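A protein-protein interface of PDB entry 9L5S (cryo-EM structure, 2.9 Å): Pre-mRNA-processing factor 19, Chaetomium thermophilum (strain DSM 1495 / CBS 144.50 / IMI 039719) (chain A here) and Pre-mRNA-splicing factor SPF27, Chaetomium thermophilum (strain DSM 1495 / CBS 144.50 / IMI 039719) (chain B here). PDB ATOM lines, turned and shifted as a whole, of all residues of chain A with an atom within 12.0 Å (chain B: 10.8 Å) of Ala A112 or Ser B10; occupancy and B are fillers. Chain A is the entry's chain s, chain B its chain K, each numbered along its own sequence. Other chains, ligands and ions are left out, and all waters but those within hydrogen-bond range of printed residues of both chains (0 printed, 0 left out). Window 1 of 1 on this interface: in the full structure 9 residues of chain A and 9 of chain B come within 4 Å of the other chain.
Among the printed residues, merely in contact across the chains: Val A116 with Glu B9 (3.3 Å), Ala A112 with Ser B10 (3.3 Å), Val A114 with Ala B26 (3.9 Å) and Ala A118 with Pro B18 (3.9 Å).
Tyr A108 touches none of the printed residues of chain B. Gln A109 touches none of the printed residues of chain B. Ala A112 touches just one residue of chain B: Ser B10. Ala A113 touches none of the printed residues of chain B. Val A114 touches just one residue of chain B: Ala B26. Of chain B, only Glu B9 (3.3 Å) comes within 4 Å of Val A116. Printed residues of chain B within 4 Å of Ala A118: Pro B18. No residue of chain A comes within 4 Å of His B8. Of chain A, only Ala A112 comes within 4 Å of Ser B10. No residue of chain A comes within 4 Å of Pro B12. Of the printed residues of chain A, Pro B18 touches Ala A118 (3.9 Å). Of the printed residues of chain A, Ala B26 touches Val A114. The nearest residue of chain B that does not touch Ala A112 is His B8 (4.3 Å). The nearest residue of chain A that does not touch Ser B10 is Val A116 (4.3 Å). The nearest printed residue of chain A that does not touch Pro B18 is Arg A115 (5.4 Å).
Of the 26 printed residues of chain B, 4 touch a printed residue of chain A. Along chain B the printed residues that touch a printed residue of chain A span positions 9 to 26.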
ATOM      1  N   LEU A 103     -28.056  31.094 -20.377  1.00  0.00           N
ATOM      2  CA  LEU A 103     -27.397  29.818 -20.639  1.00  0.00           C
ATOM      3  C   LEU A 103     -25.883  29.933 -20.505  1.00  0.00           C
ATOM      4  O   LEU A 103     -25.234  29.014 -19.995  1.00  0.00           O
ATOM      5  CB  LEU A 103     -27.775  29.310 -22.031  1.00  0.00           C
ATOM      6  N   ALA A 104     -25.304  31.047 -20.961  1.00  0.00           N
ATOM      7  CA  ALA A 104     -23.870  31.262 -20.793  1.00  0.00           C
ATOM      8  C   ALA A 104     -23.498  31.404 -19.321  1.00  0.00           C
ATOM      9  O   ALA A 104     -22.484  30.849 -18.875  1.00  0.00           O
ATOM     10  CB  ALA A 104     -23.426  32.493 -21.582  1.00  0.00           C
ATOM     11  N   THR A 105     -24.313  32.136 -18.553  1.00  0.00           N
ATOM     12  CA  THR A 105     -24.074  32.257 -17.117  1.00  0.00           C
ATOM     13  C   THR A 105     -24.211  30.909 -16.418  1.00  0.00           C
ATOM     14  O   THR A 105     -23.425  30.584 -15.520  1.00  0.00           O
ATOM     15  CB  THR A 105     -25.036  33.275 -16.506  1.00  0.00           C
ATOM     16  N   ALA A 106     -25.197  30.106 -16.829  1.00  0.00           N
ATOM     17  CA  ALA A 106     -25.381  28.780 -16.247  1.00  0.00           C
ATOM     18  C   ALA A 106     -24.225  27.851 -16.593  1.00  0.00           C
ATOM     19  O   ALA A 106     -23.802  27.048 -15.758  1.00  0.00           O
ATOM     20  CB  ALA A 106     -26.708  28.184 -16.713  1.00  0.00           C
ATOM     21  N   LEU A 107     -23.705  27.941 -17.821  1.00  0.00           N
ATOM     22  CA  LEU A 107     -22.558  27.124 -18.208  1.00  0.00           C
ATOM     23  C   LEU A 107     -21.306  27.521 -17.434  1.00  0.00           C
ATOM     24  O   LEU A 107     -20.534  26.653 -17.005  1.00  0.00           O
ATOM     25  CB  LEU A 107     -22.318  27.237 -19.713  1.00  0.00           C
ATOM     26  N   TYR A 108     -21.091  28.828 -17.245  1.00  0.00           N
ATOM     27  CA  TYR A 108     -19.955  29.283 -16.445  1.00  0.00           C
ATOM     28  C   TYR A 108     -20.090  28.844 -14.991  1.00  0.00           C
ATOM     29  O   TYR A 108     -19.110  28.406 -14.373  1.00  0.00           O
ATOM     30  CB  TYR A 108     -19.828  30.804 -16.536  1.00  0.00           C
ATOM     31  N   GLN A 109     -21.303  28.933 -14.436  1.00  0.00           N
ATOM     32  CA  GLN A 109     -21.537  28.489 -13.067  1.00  0.00           C
ATOM     33  C   GLN A 109     -21.363  26.981 -12.934  1.00  0.00           C
ATOM     34  O   GLN A 109     -20.859  26.500 -11.916  1.00  0.00           O
ATOM     35  CB  GLN A 109     -22.934  28.910 -12.610  1.00  0.00           C
ATOM     36  N   HIS A 110     -21.767  26.221 -13.956  1.00  0.00           N
ATOM     37  CA  HIS A 110     -21.593  24.773 -13.931  1.00  0.00           C
ATOM     38  C   HIS A 110     -20.122  24.389 -14.011  1.00  0.00           C
ATOM     39  O   HIS A 110     -19.686  23.454 -13.330  1.00  0.00           O
ATOM     40  CB  HIS A 110     -22.378  24.131 -15.074  1.00  0.00           C
ATOM     41  N   ASP A 111     -19.342  25.094 -14.836  1.00  0.00           N
ATOM     42  CA  ASP A 111     -17.905  24.837 -14.899  1.00  0.00           C
ATOM     43  C   ASP A 111     -17.223  25.179 -13.578  1.00  0.00           C
ATOM     44  O   ASP A 111     -16.361  24.428 -13.100  1.00  0.00           O
ATOM     45  CB  ASP A 111     -17.280  25.627 -16.048  1.00  0.00           C
ATOM     46  N   ALA A 112     -17.610  26.306 -12.967  1.00  0.00           N
ATOM     47  CA  ALA A 112     -17.052  26.681 -11.671  1.00  0.00           C
ATOM     48  C   ALA A 112     -17.437  25.680 -10.588  1.00  0.00           C
ATOM     49  O   ALA A 112     -16.611  25.329  -9.737  1.00  0.00           O
ATOM     50  CB  ALA A 112     -17.512  28.088 -11.290  1.00  0.00           C
ATOM     51  N   ALA A 113     -18.684  25.201 -10.611  1.00  0.00           N
ATOM     52  CA  ALA A 113     -19.126  24.204  -9.644  1.00  0.00           C
ATOM     53  C   ALA A 113     -18.427  22.868  -9.850  1.00  0.00           C
ATOM     54  O   ALA A 113     -18.130  22.175  -8.873  1.00  0.00           O
ATOM     55  CB  ALA A 113     -20.642  24.029  -9.725  1.00  0.00           C
ATOM     56  N   VAL A 114     -18.156  22.491 -11.103  1.00  0.00           N
ATOM     57  CA  VAL A 114     -17.418  21.261 -11.376  1.00  0.00           C
ATOM     58  C   VAL A 114     -15.988  21.367 -10.860  1.00  0.00           C
ATOM     59  O   VAL A 114     -15.459  20.421 -10.264  1.00  0.00           O
ATOM     60  CB  VAL A 114     -17.456  20.940 -12.880  1.00  0.00           C
ATOM     61  N   ARG A 115     -15.344  22.518 -11.079  1.00  0.00           N
ATOM     62  CA  ARG A 115     -13.992  22.723 -10.560  1.00  0.00           C
ATOM     63  C   ARG A 115     -13.975  22.718  -9.034  1.00  0.00           C
ATOM     64  O   ARG A 115     -13.073  22.136  -8.416  1.00  0.00           O
ATOM     65  CB  ARG A 115     -13.417  24.032 -11.100  1.00  0.00           C
ATOM     66  N   VAL A 116     -14.976  23.348  -8.412  1.00  0.00           N
ATOM     67  CA  VAL A 116     -15.058  23.383  -6.954  1.00  0.00           C
ATOM     68  C   VAL A 116     -15.321  21.991  -6.394  1.00  0.00           C
ATOM     69  O   VAL A 116     -14.780  21.619  -5.348  1.00  0.00           O
ATOM     70  CB  VAL A 116     -16.139  24.384  -6.508  1.00  0.00           C
ATOM     71  N   ILE A 117     -16.146  21.200  -7.084  1.00  0.00           N
ATOM     72  CA  ILE A 117     -16.436  19.842  -6.637  1.00  0.00           C
ATOM     73  C   ILE A 117     -15.205  18.958  -6.775  1.00  0.00           C
ATOM     74  O   ILE A 117     -14.939  18.113  -5.915  1.00  0.00           O
ATOM     75  CB  ILE A 117     -17.634  19.270  -7.416  1.00  0.00           C
ATOM     76  N   ALA A 118     -14.437  19.138  -7.855  1.00  0.00           N
ATOM     77  CA  ALA A 118     -13.192  18.392  -8.014  1.00  0.00           C
ATOM     78  C   ALA A 118     -12.185  18.751  -6.927  1.00  0.00           C
ATOM     79  O   ALA A 118     -11.531  17.865  -6.359  1.00  0.00           O
ATOM     80  CB  ALA A 118     -12.599  18.649  -9.400  1.00  0.00           C
ATOM     81  N   ARG A 119     -12.060  20.046  -6.612  1.00  0.00           N
ATOM     82  CA  ARG A 119     -11.150  20.472  -5.551  1.00  0.00           C
ATOM     83  C   ARG A 119     -11.592  19.948  -4.187  1.00  0.00           C
ATOM     84  O   ARG A 119     -10.758  19.501  -3.389  1.00  0.00           O
ATOM     85  CB  ARG A 119     -11.046  21.997  -5.532  1.00  0.00           C
ATOM     86  N   LEU A 120     -12.899  19.986  -3.909  1.00  0.00           N
ATOM     87  CA  LEU A 120     -13.413  19.485  -2.639  1.00  0.00           C
ATOM     88  C   LEU A 120     -13.240  17.976  -2.524  1.00  0.00           C
ATOM     89  O   LEU A 120     -12.920  17.466  -1.444  1.00  0.00           O
ATOM     90  CB  LEU A 120     -14.884  19.870  -2.480  1.00  0.00           C
ATOM     91  N   THR A 121     -13.445  17.245  -3.625  1.00  0.00           N
ATOM     92  CA  THR A 121     -13.232  15.803  -3.619  1.00  0.00           C
ATOM     93  C   THR A 121     -11.763  15.461  -3.404  1.00  0.00           C
ATOM     94  O   THR A 121     -11.445  14.522  -2.667  1.00  0.00           O
ATOM     95  CB  THR A 121     -13.737  15.190  -4.925  1.00  0.00           C
ATOM     96  N   ILE B   4     -28.210  34.287 -12.165  1.00  0.00           N
ATOM     97  CA  ILE B   4     -27.419  33.292 -11.446  1.00  0.00           C
ATOM     98  C   ILE B   4     -26.721  33.989 -10.282  1.00  0.00           C
ATOM     99  O   ILE B   4     -25.902  34.889 -10.486  1.00  0.00           O
ATOM    100  CB  ILE B   4     -26.407  32.603 -12.368  1.00  0.00           C
ATOM    101  N   THR B   5     -27.046  33.573  -9.060  1.00  0.00           N
ATOM    102  CA  THR B   5     -26.464  34.151  -7.856  1.00  0.00           C
ATOM    103  C   THR B   5     -25.786  33.118  -6.967  1.00  0.00           C
ATOM    104  O   THR B   5     -25.420  33.445  -5.832  1.00  0.00           O
ATOM    105  CB  THR B   5     -27.539  34.893  -7.051  1.00  0.00           C
ATOM    106  N   THR B   6     -25.617  31.887  -7.442  1.00  0.00           N
ATOM    107  CA  THR B   6     -24.960  30.859  -6.646  1.00  0.00           C
ATOM    108  C   THR B   6     -23.464  31.128  -6.553  1.00  0.00           C
ATOM    109  O   THR B   6     -22.843  31.617  -7.501  1.00  0.00           O
ATOM    110  CB  THR B   6     -25.207  29.477  -7.250  1.00  0.00           C
ATOM    111  N   VAL B   7     -22.885  30.805  -5.399  1.00  0.00           N
ATOM    112  CA  VAL B   7     -21.468  31.026  -5.133  1.00  0.00           C
ATOM    113  C   VAL B   7     -20.810  29.672  -4.913  1.00  0.00           C
ATOM    114  O   VAL B   7     -21.206  28.922  -4.013  1.00  0.00           O
ATOM    115  CB  VAL B   7     -21.250  31.945  -3.921  1.00  0.00           C
ATOM    116  N   HIS B   8     -19.809  29.363  -5.732  1.00  0.00           N
ATOM    117  CA  HIS B   8     -19.035  28.136  -5.616  1.00  0.00           C
ATOM    118  C   HIS B   8     -17.565  28.486  -5.440  1.00  0.00           C
ATOM    119  O   HIS B   8     -17.042  29.369  -6.128  1.00  0.00           O
ATOM    120  CB  HIS B   8     -19.220  27.244  -6.848  1.00  0.00           C
ATOM    121  N   GLU B   9     -16.897  27.782  -4.524  1.00  0.00           N
ATOM    122  CA  GLU B   9     -15.505  28.072  -4.175  1.00  0.00           C
ATOM    123  C   GLU B   9     -14.596  27.572  -5.296  1.00  0.00           C
ATOM    124  O   GLU B   9     -13.951  26.524  -5.208  1.00  0.00           O
ATOM    125  CB  GLU B   9     -15.145  27.440  -2.837  1.00  0.00           C
ATOM    126  N   SER B  10     -14.538  28.355  -6.370  1.00  0.00           N
ATOM    127  CA  SER B  10     -13.742  28.034  -7.546  1.00  0.00           C
ATOM    128  C   SER B  10     -12.737  29.147  -7.797  1.00  0.00           C
ATOM    129  O   SER B  10     -13.104  30.327  -7.825  1.00  0.00           O
ATOM    130  CB  SER B  10     -14.630  27.835  -8.776  1.00  0.00           C
ATOM    131  N   LEU B  11     -11.474  28.768  -7.978  1.00  0.00           N
ATOM    132  CA  LEU B  11     -10.388  29.705  -8.268  1.00  0.00           C
ATOM    133  C   LEU B  11      -9.633  29.182  -9.482  1.00  0.00           C
ATOM    134  O   LEU B  11      -8.606  28.503  -9.342  1.00  0.00           O
ATOM    135  CB  LEU B  11      -9.466  29.875  -7.061  1.00  0.00           C
ATOM    136  N   PRO B  12     -10.135  29.452 -10.692  1.00  0.00           N
ATOM    137  CA  PRO B  12      -9.461  28.945 -11.900  1.00  0.00           C
ATOM    138  C   PRO B  12      -8.056  29.488 -12.102  1.00  0.00           C
ATOM    139  O   PRO B  12      -7.191  28.766 -12.615  1.00  0.00           O
ATOM    140  CB  PRO B  12     -10.401  29.385 -13.030  1.00  0.00           C
ATOM    141  N   TYR B  13      -7.797  30.736 -11.712  1.00  0.00           N
ATOM    142  CA  TYR B  13      -6.465  31.306 -11.869  1.00  0.00           C
ATOM    143  C   TYR B  13      -5.532  30.952 -10.720  1.00  0.00           C
ATOM    144  O   TYR B  13      -4.326  31.198 -10.823  1.00  0.00           O
ATOM    145  CB  TYR B  13      -6.556  32.828 -12.007  1.00  0.00           C
ATOM    146  N   ILE B  14      -6.053  30.384  -9.636  1.00  0.00           N
ATOM    147  CA  ILE B  14      -5.270  30.076  -8.447  1.00  0.00           C
ATOM    148  C   ILE B  14      -5.145  28.572  -8.232  1.00  0.00           C
ATOM    149  O   ILE B  14      -4.038  28.040  -8.138  1.00  0.00           O
ATOM    150  CB  ILE B  14      -5.870  30.761  -7.200  1.00  0.00           C
ATOM    151  N   ASP B  15      -6.275  27.874  -8.140  1.00  0.00           N
ATOM    152  CA  ASP B  15      -6.258  26.446  -7.881  1.00  0.00           C
ATOM    153  C   ASP B  15      -5.770  25.685  -9.111  1.00  0.00           C
ATOM    154  O   ASP B  15      -5.858  26.181 -10.237  1.00  0.00           O
ATOM    155  CB  ASP B  15      -7.647  25.958  -7.479  1.00  0.00           C
ATOM    156  N   PRO B  16      -5.231  24.483  -8.912  1.00  0.00           N
ATOM    157  CA  PRO B  16      -4.741  23.700 -10.051  1.00  0.00           C
ATOM    158  C   PRO B  16      -5.877  23.225 -10.942  1.00  0.00           C
ATOM    159  O   PRO B  16      -7.013  23.036 -10.499  1.00  0.00           O
ATOM    160  CB  PRO B  16      -4.026  22.518  -9.386  1.00  0.00           C
ATOM    161  N   GLU B  17      -5.554  23.044 -12.217  1.00  0.00           N
ATOM    162  CA  GLU B  17      -6.540  22.568 -13.178  1.00  0.00           C
ATOM    163  C   GLU B  17      -6.868  21.105 -12.898  1.00  0.00           C
ATOM    164  O   GLU B  17      -5.950  20.283 -12.780  1.00  0.00           O
ATOM    165  CB  GLU B  17      -6.020  22.732 -14.604  1.00  0.00           C
ATOM    166  N   PRO B  18      -8.143  20.749 -12.762  1.00  0.00           N
ATOM    167  CA  PRO B  18      -8.493  19.350 -12.497  1.00  0.00           C
ATOM    168  C   PRO B  18      -8.187  18.452 -13.686  1.00  0.00           C
ATOM    169  O   PRO B  18      -8.244  18.869 -14.845  1.00  0.00           O
ATOM    170  CB  PRO B  18      -9.999  19.406 -12.219  1.00  0.00           C
ATOM    171  N   ARG B  23     -12.549  15.525 -13.592  1.00  0.00           N
ATOM    172  CA  ARG B  23     -13.700  16.149 -14.237  1.00  0.00           C
ATOM    173  C   ARG B  23     -14.793  15.127 -14.530  1.00  0.00           C
ATOM    174  O   ARG B  23     -15.984  15.422 -14.370  1.00  0.00           O
ATOM    175  CB  ARG B  23     -13.264  16.853 -15.521  1.00  0.00           C
ATOM    176  N   ALA B  26     -16.481  14.367 -11.222  1.00  0.00           N
ATOM    177  CA  ALA B  26     -17.372  15.465 -10.858  1.00  0.00           C
ATOM    178  C   ALA B  26     -18.644  15.449 -11.697  1.00  0.00           C
ATOM    179  O   ALA B  26     -19.741  15.702 -11.182  1.00  0.00           O
ATOM    180  CB  ALA B  26     -16.647  16.802 -11.007  1.00  0.00           C
ATOM    181  N   ILE B  30     -22.440  14.972 -10.381  1.00  0.00           N
ATOM    182  CA  ILE B  30     -23.504  15.896 -10.769  1.00  0.00           C
ATOM    183  C   ILE B  30     -24.671  15.142 -11.397  1.00  0.00           C
ATOM    184  O   ILE B  30     -25.838  15.471 -11.158  1.00  0.00           O
ATOM    185  CB  ILE B  30     -22.952  16.976 -11.715  1.00  0.00           C
ATOM    186  N   ARG B 174      -9.389  39.892 -12.615  1.00  0.00           N
ATOM    187  CA  ARG B 174      -9.788  38.701 -11.874  1.00  0.00           C
ATOM    188  C   ARG B 174      -8.620  37.740 -11.702  1.00  0.00           C
ATOM    189  O   ARG B 174      -8.459  37.141 -10.634  1.00  0.00           O
ATOM    190  CB  ARG B 174     -10.952  38.010 -12.582  1.00  0.00           C
ATOM    191  N   GLN B 175      -7.786  37.593 -12.737  1.00  0.00           N
ATOM    192  CA  GLN B 175      -6.623  36.718 -12.652  1.00  0.00           C
ATOM    193  C   GLN B 175      -5.614  37.229 -11.631  1.00  0.00           C
ATOM    194  O   GLN B 175      -5.054  36.442 -10.863  1.00  0.00           O
ATOM    195  CB  GLN B 175      -5.970  36.579 -14.027  1.00  0.00           C
ATOM    196  N   MET B 177      -6.235  39.267  -8.962  1.00  0.00           N
ATOM    197  CA  MET B 177      -6.806  39.117  -7.626  1.00  0.00           C
ATOM    198  C   MET B 177      -6.812  37.656  -7.189  1.00  0.00           C
ATOM    199  O   MET B 177      -6.493  37.343  -6.033  1.00  0.00           O
ATOM    200  CB  MET B 177      -8.221  39.694  -7.592  1.00  0.00           C
ATOM    201  N   GLN B 178      -7.153  36.748  -8.109  1.00  0.00           N
ATOM    202  CA  GLN B 178      -7.149  35.324  -7.801  1.00  0.00           C
ATOM    203  C   GLN B 178      -5.741  34.818  -7.526  1.00  0.00           C
ATOM    204  O   GLN B 178      -5.550  33.970  -6.656  1.00  0.00           O
ATOM    205  CB  GLN B 178      -7.789  34.539  -8.945  1.00  0.00           C
ATOM    206  N   GLU B 179      -4.740  35.331  -8.250  1.00  0.00           N
ATOM    207  CA  GLU B 179      -3.362  34.914  -8.014  1.00  0.00           C
ATOM    208  C   GLU B 179      -2.869  35.366  -6.644  1.00  0.00           C
ATOM    209  O   GLU B 179      -2.216  34.594  -5.931  1.00  0.00           O
ATOM    210  CB  GLU B 179      -2.453  35.458  -9.117  1.00  0.00           C
ATOM    211  N   ALA B 181      -4.797  36.069  -3.978  1.00  0.00           N
ATOM    212  CA  ALA B 181      -5.544  35.305  -2.984  1.00  0.00           C
ATOM    213  C   ALA B 181      -5.068  33.859  -2.922  1.00  0.00           C
ATOM    214  O   ALA B 181      -5.002  33.269  -1.840  1.00  0.00           O
ATOM    215  CB  ALA B 181      -7.040  35.366  -3.290  1.00  0.00           C
ATOM    216  N   GLY B 182      -4.724  33.277  -4.072  1.00  0.00           N
ATOM    217  CA  GLY B 182      -4.231  31.912  -4.092  1.00  0.00           C
ATOM    218  C   GLY B 182      -2.860  31.768  -3.466  1.00  0.00           C
ATOM    219  O   GLY B 182      -2.582  30.769  -2.803  1.00  0.00           O
ATOM    220  N   LEU B 185      -3.530  31.991   0.251  1.00  0.00           N
ATOM    221  CA  LEU B 185      -4.196  30.787   0.734  1.00  0.00           C
ATOM    222  C   LEU B 185      -3.262  29.583   0.713  1.00  0.00           C
ATOM    223  O   LEU B 185      -3.349  28.716   1.587  1.00  0.00           O
ATOM    224  CB  LEU B 185      -5.446  30.511  -0.100  1.00  0.00           C
